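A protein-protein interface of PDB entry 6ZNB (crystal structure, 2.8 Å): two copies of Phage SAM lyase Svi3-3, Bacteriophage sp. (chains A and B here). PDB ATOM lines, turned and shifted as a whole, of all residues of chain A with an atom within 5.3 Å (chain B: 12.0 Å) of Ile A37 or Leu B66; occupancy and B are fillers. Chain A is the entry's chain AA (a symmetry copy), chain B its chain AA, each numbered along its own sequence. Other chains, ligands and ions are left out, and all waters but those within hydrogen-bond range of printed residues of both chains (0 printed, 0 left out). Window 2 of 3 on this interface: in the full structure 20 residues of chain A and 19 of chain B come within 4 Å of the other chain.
Of chain B, only Val B57 (3.8 Å) comes within 4 Å of Val A33.
Ile A37 touches just these residues of chain B: Val B57 (3.5 Å) and Leu B66 (3.7 Å).
No residue of chain B comes within 4 Å of Ile A39.
Printed residues of chain A within 4 Å of Val B57: Val A33 (3.8 Å), Ile A37 (3.5 Å), Pro A47 (3.9 Å) and Asp A48 (3.2 Å).
Of the printed residues of chain A, Tyr B58 touches Asp A48 (3.5 Å).
Printed residues of chain A within 4 Å of Thr B59: Asp A48 (3.1 Å).
The nearest residue of chain B that does not touch Ile A37 is Thr B68 (5.7 Å).
The backbone carbonyl oxygen of Gly B22 sits at hydrogen-bond distance from the side-chain hydroxyl of Tyr B58, 3.4 Å away.
The backbone carbonyl oxygen (O) of Tyr B58 lies within hydrogen-bond range of the backbone NH (N) of Val B67, at 2.9 Å.
Along chain A the printed residues that touch a printed residue of chain B span positions 33 to 48.
Printed residues of chain B that touch a printed residue of chain A: Val B57, Tyr B58, Thr B59 and Leu B66.
Hydrophobic or aromatic side chains of chain B that line the printed part of chain A: Val B57 and Leu B66.
N of Thr B59 sits at hydrogen-bond distance from OD2 of Asp A48, at 3.1 Å.
Among the printed residues, pairs that only touch across the chains: Asp A48 with Val B57 (3.2 Å), Asp A48 with Tyr B58 (3.5 Å), Ile A37 with Val B57 (3.5 Å), Ile A37 with Leu B66 (3.7 Å), Pro A47 with Leu B66 (3.7 Å), Asp A48 with Leu B66 (3.8 Å), Val A33 with Val B57 (3.8 Å) and Pro A47 with Val B57 (3.9 Å).
No position is printed for both chains.
Of the 9 pairs that touch across the chains among the printed residues, none has its exchanged pair printed and touching as well.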
ATOM      1  N   VAL A  32     -17.262  10.025 -21.345  1.00  0.00           N
ATOM      2  CA  VAL A  32     -17.376  11.113 -20.381  1.00  0.00           C
ATOM      3  C   VAL A  32     -16.117  11.228 -19.529  1.00  0.00           C
ATOM      4  O   VAL A  32     -15.673  12.337 -19.214  1.00  0.00           O
ATOM      5  CB  VAL A  32     -18.642  10.923 -19.525  1.00  0.00           C
ATOM      6  CG1 VAL A  32     -18.648  11.881 -18.342  1.00  0.00           C
ATOM      7  CG2 VAL A  32     -19.891  11.119 -20.378  1.00  0.00           C
ATOM      8  N   VAL A  33     -15.500  10.101 -19.161  1.00  0.00           N
ATOM      9  CA  VAL A  33     -14.303  10.172 -18.326  1.00  0.00           C
ATOM     10  C   VAL A  33     -13.130  10.738 -19.118  1.00  0.00           C
ATOM     11  O   VAL A  33     -12.402  11.608 -18.629  1.00  0.00           O
ATOM     12  CB  VAL A  33     -13.971   8.796 -17.713  1.00  0.00           C
ATOM     13  CG1 VAL A  33     -14.015   7.710 -18.753  1.00  0.00           C
ATOM     14  CG2 VAL A  33     -12.600   8.825 -17.056  1.00  0.00           C
ATOM     15  N   LYS A  34     -12.936  10.272 -20.356  1.00  0.00           N
ATOM     16  CA  LYS A  34     -11.846  10.799 -21.176  1.00  0.00           C
ATOM     17  C   LYS A  34     -12.026  12.289 -21.441  1.00  0.00           C
ATOM     18  O   LYS A  34     -11.053  13.053 -21.429  1.00  0.00           O
ATOM     19  CB  LYS A  34     -11.753  10.028 -22.493  1.00  0.00           C
ATOM     20  CG  LYS A  34     -11.248   8.600 -22.345  1.00  0.00           C
ATOM     21  CD  LYS A  34     -10.798   8.025 -23.680  1.00  0.00           C
ATOM     22  CE  LYS A  34     -10.242   6.619 -23.516  1.00  0.00           C
ATOM     23  NZ  LYS A  34      -9.624   6.112 -24.773  1.00  0.00           N
ATOM     24  N   ASP A  35     -13.266  12.724 -21.674  1.00  0.00           N
ATOM     25  CA  ASP A  35     -13.526  14.140 -21.901  1.00  0.00           C
ATOM     26  C   ASP A  35     -13.454  14.955 -20.615  1.00  0.00           C
ATOM     27  O   ASP A  35     -13.199  16.163 -20.676  1.00  0.00           O
ATOM     28  CB  ASP A  35     -14.893  14.319 -22.563  1.00  0.00           C
ATOM     29  CG  ASP A  35     -15.149  15.749 -22.992  1.00  0.00           C
ATOM     30  OD1 ASP A  35     -15.862  16.466 -22.261  1.00  0.00           O
ATOM     31  OD2 ASP A  35     -14.636  16.155 -24.057  1.00  0.00           O
ATOM     32  N   THR A  36     -13.669  14.327 -19.456  1.00  0.00           N
ATOM     33  CA  THR A  36     -13.579  15.052 -18.193  1.00  0.00           C
ATOM     34  C   THR A  36     -12.129  15.312 -17.800  1.00  0.00           C
ATOM     35  O   THR A  36     -11.808  16.394 -17.294  1.00  0.00           O
ATOM     36  CB  THR A  36     -14.307  14.280 -17.090  1.00  0.00           C
ATOM     37  OG1 THR A  36     -15.708  14.227 -17.393  1.00  0.00           O
ATOM     38  CG2 THR A  36     -14.120  14.957 -15.741  1.00  0.00           C
ATOM     39  N   ILE A  37     -11.240  14.341 -18.027  1.00  0.00           N
ATOM     40  CA  ILE A  37      -9.817  14.576 -17.782  1.00  0.00           C
ATOM     41  C   ILE A  37      -9.305  15.699 -18.673  1.00  0.00           C
ATOM     42  O   ILE A  37      -8.527  16.555 -18.234  1.00  0.00           O
ATOM     43  CB  ILE A  37      -9.004  13.287 -17.998  1.00  0.00           C
ATOM     44  CG1 ILE A  37      -9.679  12.084 -17.341  1.00  0.00           C
ATOM     45  CG2 ILE A  37      -7.592  13.458 -17.460  1.00  0.00           C
ATOM     46  CD1 ILE A  37      -8.904  10.800 -17.528  1.00  0.00           C
ATOM     47  N   ALA A  38      -9.732  15.711 -19.939  1.00  0.00           N
ATOM     48  CA  ALA A  38      -9.238  16.708 -20.882  1.00  0.00           C
ATOM     49  C   ALA A  38      -9.627  18.118 -20.458  1.00  0.00           C
ATOM     50  O   ALA A  38      -8.813  19.045 -20.537  1.00  0.00           O
ATOM     51  CB  ALA A  38      -9.763  16.407 -22.285  1.00  0.00           C
ATOM     52  N   ILE A  39     -10.868  18.298 -20.000  1.00  0.00           N
ATOM     53  CA  ILE A  39     -11.332  19.624 -19.608  1.00  0.00           C
ATOM     54  C   ILE A  39     -10.569  20.116 -18.384  1.00  0.00           C
ATOM     55  O   ILE A  39     -10.032  21.230 -18.374  1.00  0.00           O
ATOM     56  CB  ILE A  39     -12.850  19.609 -19.353  1.00  0.00           C
ATOM     57  CG1 ILE A  39     -13.610  19.399 -20.665  1.00  0.00           C
ATOM     58  CG2 ILE A  39     -13.289  20.897 -18.677  1.00  0.00           C
ATOM     59  CD1 ILE A  39     -15.073  19.072 -20.471  1.00  0.00           C
ATOM     60  N   ARG A  40     -10.507  19.293 -17.335  1.00  0.00           N
ATOM     61  CA  ARG A  40      -9.850  19.710 -16.104  1.00  0.00           C
ATOM     62  C   ARG A  40      -8.341  19.853 -16.269  1.00  0.00           C
ATOM     63  O   ARG A  40      -7.720  20.608 -15.515  1.00  0.00           O
ATOM     64  CB  ARG A  40     -10.180  18.726 -14.979  1.00  0.00           C
ATOM     65  CG  ARG A  40     -11.627  18.816 -14.498  1.00  0.00           C
ATOM     66  CD  ARG A  40     -12.035  17.587 -13.697  1.00  0.00           C
ATOM     67  NE  ARG A  40     -11.341  17.513 -12.413  1.00  0.00           N
ATOM     68  CZ  ARG A  40     -11.592  18.304 -11.373  1.00  0.00           C
ATOM     69  NH1 ARG A  40     -12.545  19.224 -11.441  1.00  0.00           N
ATOM     70  NH2 ARG A  40     -10.895  18.162 -10.253  1.00  0.00           N
ATOM     71  N   LYS A  41      -7.742  19.154 -17.237  1.00  0.00           N
ATOM     72  CA  LYS A  41      -6.340  19.394 -17.564  1.00  0.00           C
ATOM     73  C   LYS A  41      -6.136  20.826 -18.042  1.00  0.00           C
ATOM     74  O   LYS A  41      -5.188  21.504 -17.630  1.00  0.00           O
ATOM     75  CB  LYS A  41      -5.873  18.401 -18.629  1.00  0.00           C
ATOM     76  CG  LYS A  41      -5.134  17.190 -18.090  1.00  0.00           C
ATOM     77  CD  LYS A  41      -4.565  16.363 -19.231  1.00  0.00           C
ATOM     78  CE  LYS A  41      -3.568  15.333 -18.735  1.00  0.00           C
ATOM     79  NZ  LYS A  41      -2.859  14.674 -19.866  1.00  0.00           N
ATOM     80  N   ARG A  42      -7.025  21.303 -18.918  1.00  0.00           N
ATOM     81  CA  ARG A  42      -6.951  22.676 -19.403  1.00  0.00           C
ATOM     82  C   ARG A  42      -7.288  23.689 -18.319  1.00  0.00           C
ATOM     83  O   ARG A  42      -6.933  24.865 -18.457  1.00  0.00           O
ATOM     84  CB  ARG A  42      -7.886  22.860 -20.599  1.00  0.00           C
ATOM     85  CG  ARG A  42      -7.708  21.818 -21.691  1.00  0.00           C
ATOM     86  CD  ARG A  42      -8.525  22.156 -22.930  1.00  0.00           C
ATOM     87  NE  ARG A  42      -8.797  20.969 -23.736  1.00  0.00           N
ATOM     88  CZ  ARG A  42     -10.000  20.418 -23.878  1.00  0.00           C
ATOM     89  NH1 ARG A  42     -11.052  20.949 -23.270  1.00  0.00           N
ATOM     90  NH2 ARG A  42     -10.150  19.338 -24.632  1.00  0.00           N
ATOM     91  N   PRO A  47      -6.809  16.493 -12.563  1.00  0.00           N
ATOM     92  CA  PRO A  47      -8.089  16.016 -13.101  1.00  0.00           C
ATOM     93  C   PRO A  47      -8.656  14.817 -12.357  1.00  0.00           C
ATOM     94  O   PRO A  47      -9.520  14.108 -12.883  1.00  0.00           O
ATOM     95  CB  PRO A  47      -7.734  15.661 -14.549  1.00  0.00           C
ATOM     96  CG  PRO A  47      -6.305  15.235 -14.470  1.00  0.00           C
ATOM     97  CD  PRO A  47      -5.669  16.106 -13.413  1.00  0.00           C
ATOM     98  N   ASP A  48      -8.194  14.592 -11.129  1.00  0.00           N
ATOM     99  CA  ASP A  48      -8.600  13.415 -10.369  1.00  0.00           C
ATOM    100  C   ASP A  48     -10.095  13.446 -10.075  1.00  0.00           C
ATOM    101  O   ASP A  48     -10.600  14.398  -9.473  1.00  0.00           O
ATOM    102  CB  ASP A  48      -7.802  13.327  -9.069  1.00  0.00           C
ATOM    103  CG  ASP A  48      -6.311  13.162  -9.308  1.00  0.00           C
ATOM    104  OD1 ASP A  48      -5.861  13.373 -10.456  1.00  0.00           O
ATOM    105  OD2 ASP A  48      -5.589  12.813  -8.351  1.00  0.00           O
ATOM    106  N   ASN B  20      -5.893  -1.718  -9.013  1.00  0.00           N
ATOM    107  CA  ASN B  20      -4.651  -1.760  -9.771  1.00  0.00           C
ATOM    108  C   ASN B  20      -3.457  -1.908  -8.838  1.00  0.00           C
ATOM    109  O   ASN B  20      -3.413  -1.291  -7.768  1.00  0.00           O
ATOM    110  CB  ASN B  20      -4.471  -0.492 -10.613  1.00  0.00           C
ATOM    111  CG  ASN B  20      -5.367  -0.462 -11.834  1.00  0.00           C
ATOM    112  OD1 ASN B  20      -6.269  -1.284 -11.980  1.00  0.00           O
ATOM    113  ND2 ASN B  20      -5.114   0.487 -12.726  1.00  0.00           N
ATOM    114  N   VAL B  21      -2.484  -2.719  -9.244  1.00  0.00           N
ATOM    115  CA  VAL B  21      -1.159  -2.691  -8.635  1.00  0.00           C
ATOM    116  C   VAL B  21      -0.307  -1.767  -9.500  1.00  0.00           C
ATOM    117  O   VAL B  21       0.002  -2.085 -10.658  1.00  0.00           O
ATOM    118  CB  VAL B  21      -0.537  -4.091  -8.484  1.00  0.00           C
ATOM    119  CG1 VAL B  21      -1.187  -4.834  -7.325  1.00  0.00           C
ATOM    120  CG2 VAL B  21      -0.567  -4.911  -9.777  1.00  0.00           C
ATOM    121  N   GLY B  22       0.029  -0.595  -8.957  1.00  0.00           N
ATOM    122  CA  GLY B  22       0.700   0.412  -9.753  1.00  0.00           C
ATOM    123  C   GLY B  22      -0.204   0.912 -10.860  1.00  0.00           C
ATOM    124  O   GLY B  22      -0.973   1.861 -10.665  1.00  0.00           O
ATOM    125  N   ASP B  23      -0.141   0.265 -12.028  1.00  0.00           N
ATOM    126  CA  ASP B  23      -0.989   0.656 -13.146  1.00  0.00           C
ATOM    127  C   ASP B  23      -1.610  -0.537 -13.863  1.00  0.00           C
ATOM    128  O   ASP B  23      -2.178  -0.355 -14.945  1.00  0.00           O
ATOM    129  CB  ASP B  23      -0.192   1.501 -14.146  1.00  0.00           C
ATOM    130  CG  ASP B  23       1.005   0.761 -14.712  1.00  0.00           C
ATOM    131  OD1 ASP B  23       1.826   0.249 -13.922  1.00  0.00           O
ATOM    132  OD2 ASP B  23       1.119   0.686 -15.953  1.00  0.00           O
ATOM    133  N   LYS B  24      -1.532  -1.745 -13.300  1.00  0.00           N
ATOM    134  CA  LYS B  24      -2.025  -2.937 -13.975  1.00  0.00           C
ATOM    135  C   LYS B  24      -3.345  -3.376 -13.362  1.00  0.00           C
ATOM    136  O   LYS B  24      -3.396  -3.617 -12.144  1.00  0.00           O
ATOM    137  CB  LYS B  24      -1.001  -4.062 -13.878  1.00  0.00           C
ATOM    138  CG  LYS B  24      -1.372  -5.322 -14.649  1.00  0.00           C
ATOM    139  CD  LYS B  24      -1.396  -5.072 -16.148  1.00  0.00           C
ATOM    140  CE  LYS B  24      -2.119  -6.192 -16.878  1.00  0.00           C
ATOM    141  NZ  LYS B  24      -3.561  -6.247 -16.508  1.00  0.00           N
ATOM    142  N   PRO B  25      -4.423  -3.481 -14.141  1.00  0.00           N
ATOM    143  CA  PRO B  25      -5.661  -4.067 -13.610  1.00  0.00           C
ATOM    144  C   PRO B  25      -5.411  -5.481 -13.108  1.00  0.00           C
ATOM    145  O   PRO B  25      -4.845  -6.319 -13.814  1.00  0.00           O
ATOM    146  CB  PRO B  25      -6.608  -4.048 -14.814  1.00  0.00           C
ATOM    147  CG  PRO B  25      -6.101  -2.932 -15.661  1.00  0.00           C
ATOM    148  CD  PRO B  25      -4.605  -2.956 -15.504  1.00  0.00           C
ATOM    149  N   ARG B  55     -15.379   3.957 -11.727  1.00  0.00           N
ATOM    150  CA  ARG B  55     -14.211   4.240 -12.546  1.00  0.00           C
ATOM    151  C   ARG B  55     -13.429   5.364 -11.885  1.00  0.00           C
ATOM    152  O   ARG B  55     -14.016   6.332 -11.390  1.00  0.00           O
ATOM    153  CB  ARG B  55     -14.610   4.638 -13.969  1.00  0.00           C
ATOM    154  CG  ARG B  55     -15.471   3.615 -14.686  1.00  0.00           C
ATOM    155  CD  ARG B  55     -14.916   3.300 -16.066  1.00  0.00           C
ATOM    156  NE  ARG B  55     -13.814   2.344 -16.002  1.00  0.00           N
ATOM    157  CZ  ARG B  55     -12.578   2.599 -16.417  1.00  0.00           C
ATOM    158  NH1 ARG B  55     -12.280   3.787 -16.929  1.00  0.00           N
ATOM    159  NH2 ARG B  55     -11.638   1.669 -16.320  1.00  0.00           N
ATOM    160  N   GLY B  56     -12.109   5.235 -11.859  1.00  0.00           N
ATOM    161  CA  GLY B  56     -11.275   6.168 -11.137  1.00  0.00           C
ATOM    162  C   GLY B  56     -10.177   6.760 -12.010  1.00  0.00           C
ATOM    163  O   GLY B  56      -9.690   6.125 -12.941  1.00  0.00           O
ATOM    164  N   VAL B  57      -9.815   7.994 -11.681  1.00  0.00           N
ATOM    165  CA  VAL B  57      -8.703   8.692 -12.321  1.00  0.00           C
ATOM    166  C   VAL B  57      -7.951   9.448 -11.236  1.00  0.00           C
ATOM    167  O   VAL B  57      -8.546  10.259 -10.516  1.00  0.00           O
ATOM    168  CB  VAL B  57      -9.171   9.655 -13.426  1.00  0.00           C
ATOM    169  CG1 VAL B  57      -8.063  10.628 -13.786  1.00  0.00           C
ATOM    170  CG2 VAL B  57      -9.621   8.875 -14.649  1.00  0.00           C
ATOM    171  N   TYR B  58      -6.652   9.183 -11.111  1.00  0.00           N
ATOM    172  CA  TYR B  58      -5.856   9.753 -10.035  1.00  0.00           C
ATOM    173  C   TYR B  58      -4.435   9.986 -10.526  1.00  0.00           C
ATOM    174  O   TYR B  58      -4.005   9.415 -11.532  1.00  0.00           O
ATOM    175  CB  TYR B  58      -5.846   8.839  -8.801  1.00  0.00           C
ATOM    176  CG  TYR B  58      -5.294   7.455  -9.074  1.00  0.00           C
ATOM    177  CD1 TYR B  58      -3.962   7.151  -8.816  1.00  0.00           C
ATOM    178  CD2 TYR B  58      -6.102   6.454  -9.597  1.00  0.00           C
ATOM    179  CE1 TYR B  58      -3.454   5.889  -9.067  1.00  0.00           C
ATOM    180  CE2 TYR B  58      -5.601   5.191  -9.852  1.00  0.00           C
ATOM    181  CZ  TYR B  58      -4.277   4.913  -9.585  1.00  0.00           C
ATOM    182  OH  TYR B  58      -3.773   3.657  -9.837  1.00  0.00           O
ATOM    183  N   THR B  59      -3.713  10.841  -9.805  1.00  0.00           N
ATOM    184  CA  THR B  59      -2.284  11.030 -10.040  1.00  0.00           C
ATOM    185  C   THR B  59      -1.470  10.357  -8.939  1.00  0.00           C
ATOM    186  O   THR B  59      -1.737  10.545  -7.754  1.00  0.00           O
ATOM    187  CB  THR B  59      -1.895  12.522 -10.110  1.00  0.00           C
ATOM    188  OG1 THR B  59      -2.465  13.218  -8.995  1.00  0.00           O
ATOM    189  CG2 THR B  59      -2.369  13.161 -11.413  1.00  0.00           C
ATOM    190  N   GLY B  64       5.316  10.237 -10.182  1.00  0.00           N
ATOM    191  CA  GLY B  64       3.897  10.546 -10.207  1.00  0.00           C
ATOM    192  C   GLY B  64       3.341  10.750 -11.606  1.00  0.00           C
ATOM    193  O   GLY B  64       3.870  11.545 -12.384  1.00  0.00           O
ATOM    194  N   GLN B  65       2.268  10.026 -11.923  1.00  0.00           N
ATOM    195  CA  GLN B  65       1.603  10.135 -13.213  1.00  0.00           C
ATOM    196  C   GLN B  65       0.123   9.820 -13.020  1.00  0.00           C
ATOM    197  O   GLN B  65      -0.318   9.462 -11.925  1.00  0.00           O
ATOM    198  CB  GLN B  65       2.255   9.208 -14.246  1.00  0.00           C
ATOM    199  CG  GLN B  65       3.310   9.886 -15.112  1.00  0.00           C
ATOM    200  CD  GLN B  65       2.711  10.800 -16.167  1.00  0.00           C
ATOM    201  OE1 GLN B  65       1.492  10.951 -16.259  1.00  0.00           O
ATOM    202  NE2 GLN B  65       3.570  11.419 -16.969  1.00  0.00           N
ATOM    203  N   LEU B  66      -0.643   9.944 -14.102  1.00  0.00           N
ATOM    204  CA  LEU B  66      -2.097   9.812 -14.066  1.00  0.00           C
ATOM    205  C   LEU B  66      -2.521   8.418 -14.524  1.00  0.00           C
ATOM    206  O   LEU B  66      -2.278   8.039 -15.673  1.00  0.00           O
ATOM    207  CB  LEU B  66      -2.753  10.883 -14.938  1.00  0.00           C
ATOM    208  CG  LEU B  66      -4.285  10.978 -14.896  1.00  0.00           C
ATOM    209  CD1 LEU B  66      -4.719  11.961 -13.809  1.00  0.00           C
ATOM    210  CD2 LEU B  66      -4.838  11.368 -16.258  1.00  0.00           C
ATOM    211  N   VAL B  67      -3.163   7.668 -13.630  1.00  0.00           N
ATOM    212  CA  VAL B  67      -3.626   6.314 -13.909  1.00  0.00           C
ATOM    213  C   VAL B  67      -5.151   6.310 -13.917  1.00  0.00           C
ATOM    214  O   VAL B  67      -5.789   7.035 -13.147  1.00  0.00           O
ATOM    215  CB  VAL B  67      -3.078   5.315 -12.869  1.00  0.00           C
ATOM    216  CG1 VAL B  67      -3.673   3.919 -13.079  1.00  0.00           C
ATOM    217  CG2 VAL B  67      -1.564   5.252 -12.927  1.00  0.00           C
ATOM    218  N   THR B  68      -5.728   5.507 -14.805  1.00  0.00           N
ATOM    219  CA  THR B  68      -7.159   5.232 -14.804  1.00  0.00           C
ATOM    220  C   THR B  68      -7.373   3.809 -14.300  1.00  0.00           C
ATOM    221  O   THR B  68      -6.823   2.854 -14.863  1.00  0.00           O
ATOM    222  CB  THR B  68      -7.772   5.421 -16.194  1.00  0.00           C
ATOM    223  OG1 THR B  68      -9.087   4.846 -16.220  1.00  0.00           O
ATOM    224  CG2 THR B  68      -6.907   4.768 -17.272  1.00  0.00           C
ATOM    225  N   GLU B  69      -8.156   3.670 -13.233  1.00  0.00           N
ATOM    226  CA  GLU B  69      -8.358   2.380 -12.594  1.00  0.00           C
ATOM    227  C   GLU B  69      -9.829   2.188 -12.262  1.00  0.00           C
ATOM    228  O   GLU B  69     -10.578   3.153 -12.089  1.00  0.00           O
ATOM    229  CB  GLU B  69      -7.526   2.247 -11.308  1.00  0.00           C
ATOM    230  CG  GLU B  69      -8.179   2.868 -10.080  1.00  0.00           C
ATOM    231  CD  GLU B  69      -7.412   2.587  -8.800  1.00  0.00           C
ATOM    232  OE1 GLU B  69      -6.532   1.699  -8.811  1.00  0.00           O
ATOM    233  OE2 GLU B  69      -7.688   3.257  -7.782  1.00  0.00           O
ATOM    234  N   ASN B  70     -10.235   0.925 -12.187  1.00  0.00           N
ATOM    235  CA  ASN B  70     -11.504   0.574 -11.577  1.00  0.00           C
ATOM    236  C   ASN B  70     -11.338   0.547 -10.064  1.00  0.00           C
ATOM    237  O   ASN B  70     -10.293   0.141  -9.547  1.00  0.00           O
ATOM    238  CB  ASN B  70     -11.990  -0.788 -12.074  1.00  0.00           C
ATOM    239  CG  ASN B  70     -12.461  -0.753 -13.515  1.00  0.00           C
ATOM    240  OD1 ASN B  70     -12.786   0.306 -14.051  1.00  0.00           O
ATOM    241  ND2 ASN B  70     -12.506  -1.919 -14.149  1.00  0.00           N
ATOM    242  N   GLU B 105      -1.442   1.406  -2.551  1.00  0.00           N
ATOM    243  CA  GLU B 105      -0.604   2.452  -1.979  1.00  0.00           C
ATOM    244  C   GLU B 105      -1.377   3.278  -0.961  1.00  0.00           C
ATOM    245  O   GLU B 105      -0.792   3.774   0.009  1.00  0.00           O
ATOM    246  CB  GLU B 105      -0.053   3.347  -3.089  1.00  0.00           C
ATOM    247  CG  GLU B 105       0.809   4.500  -2.597  1.00  0.00           C
ATOM    248  CD  GLU B 105       1.211   5.445  -3.710  1.00  0.00           C
ATOM    249  OE1 GLU B 105       0.515   5.476  -4.748  1.00  0.00           O
ATOM    250  OE2 GLU B 105       2.225   6.159  -3.549  1.00  0.00           O
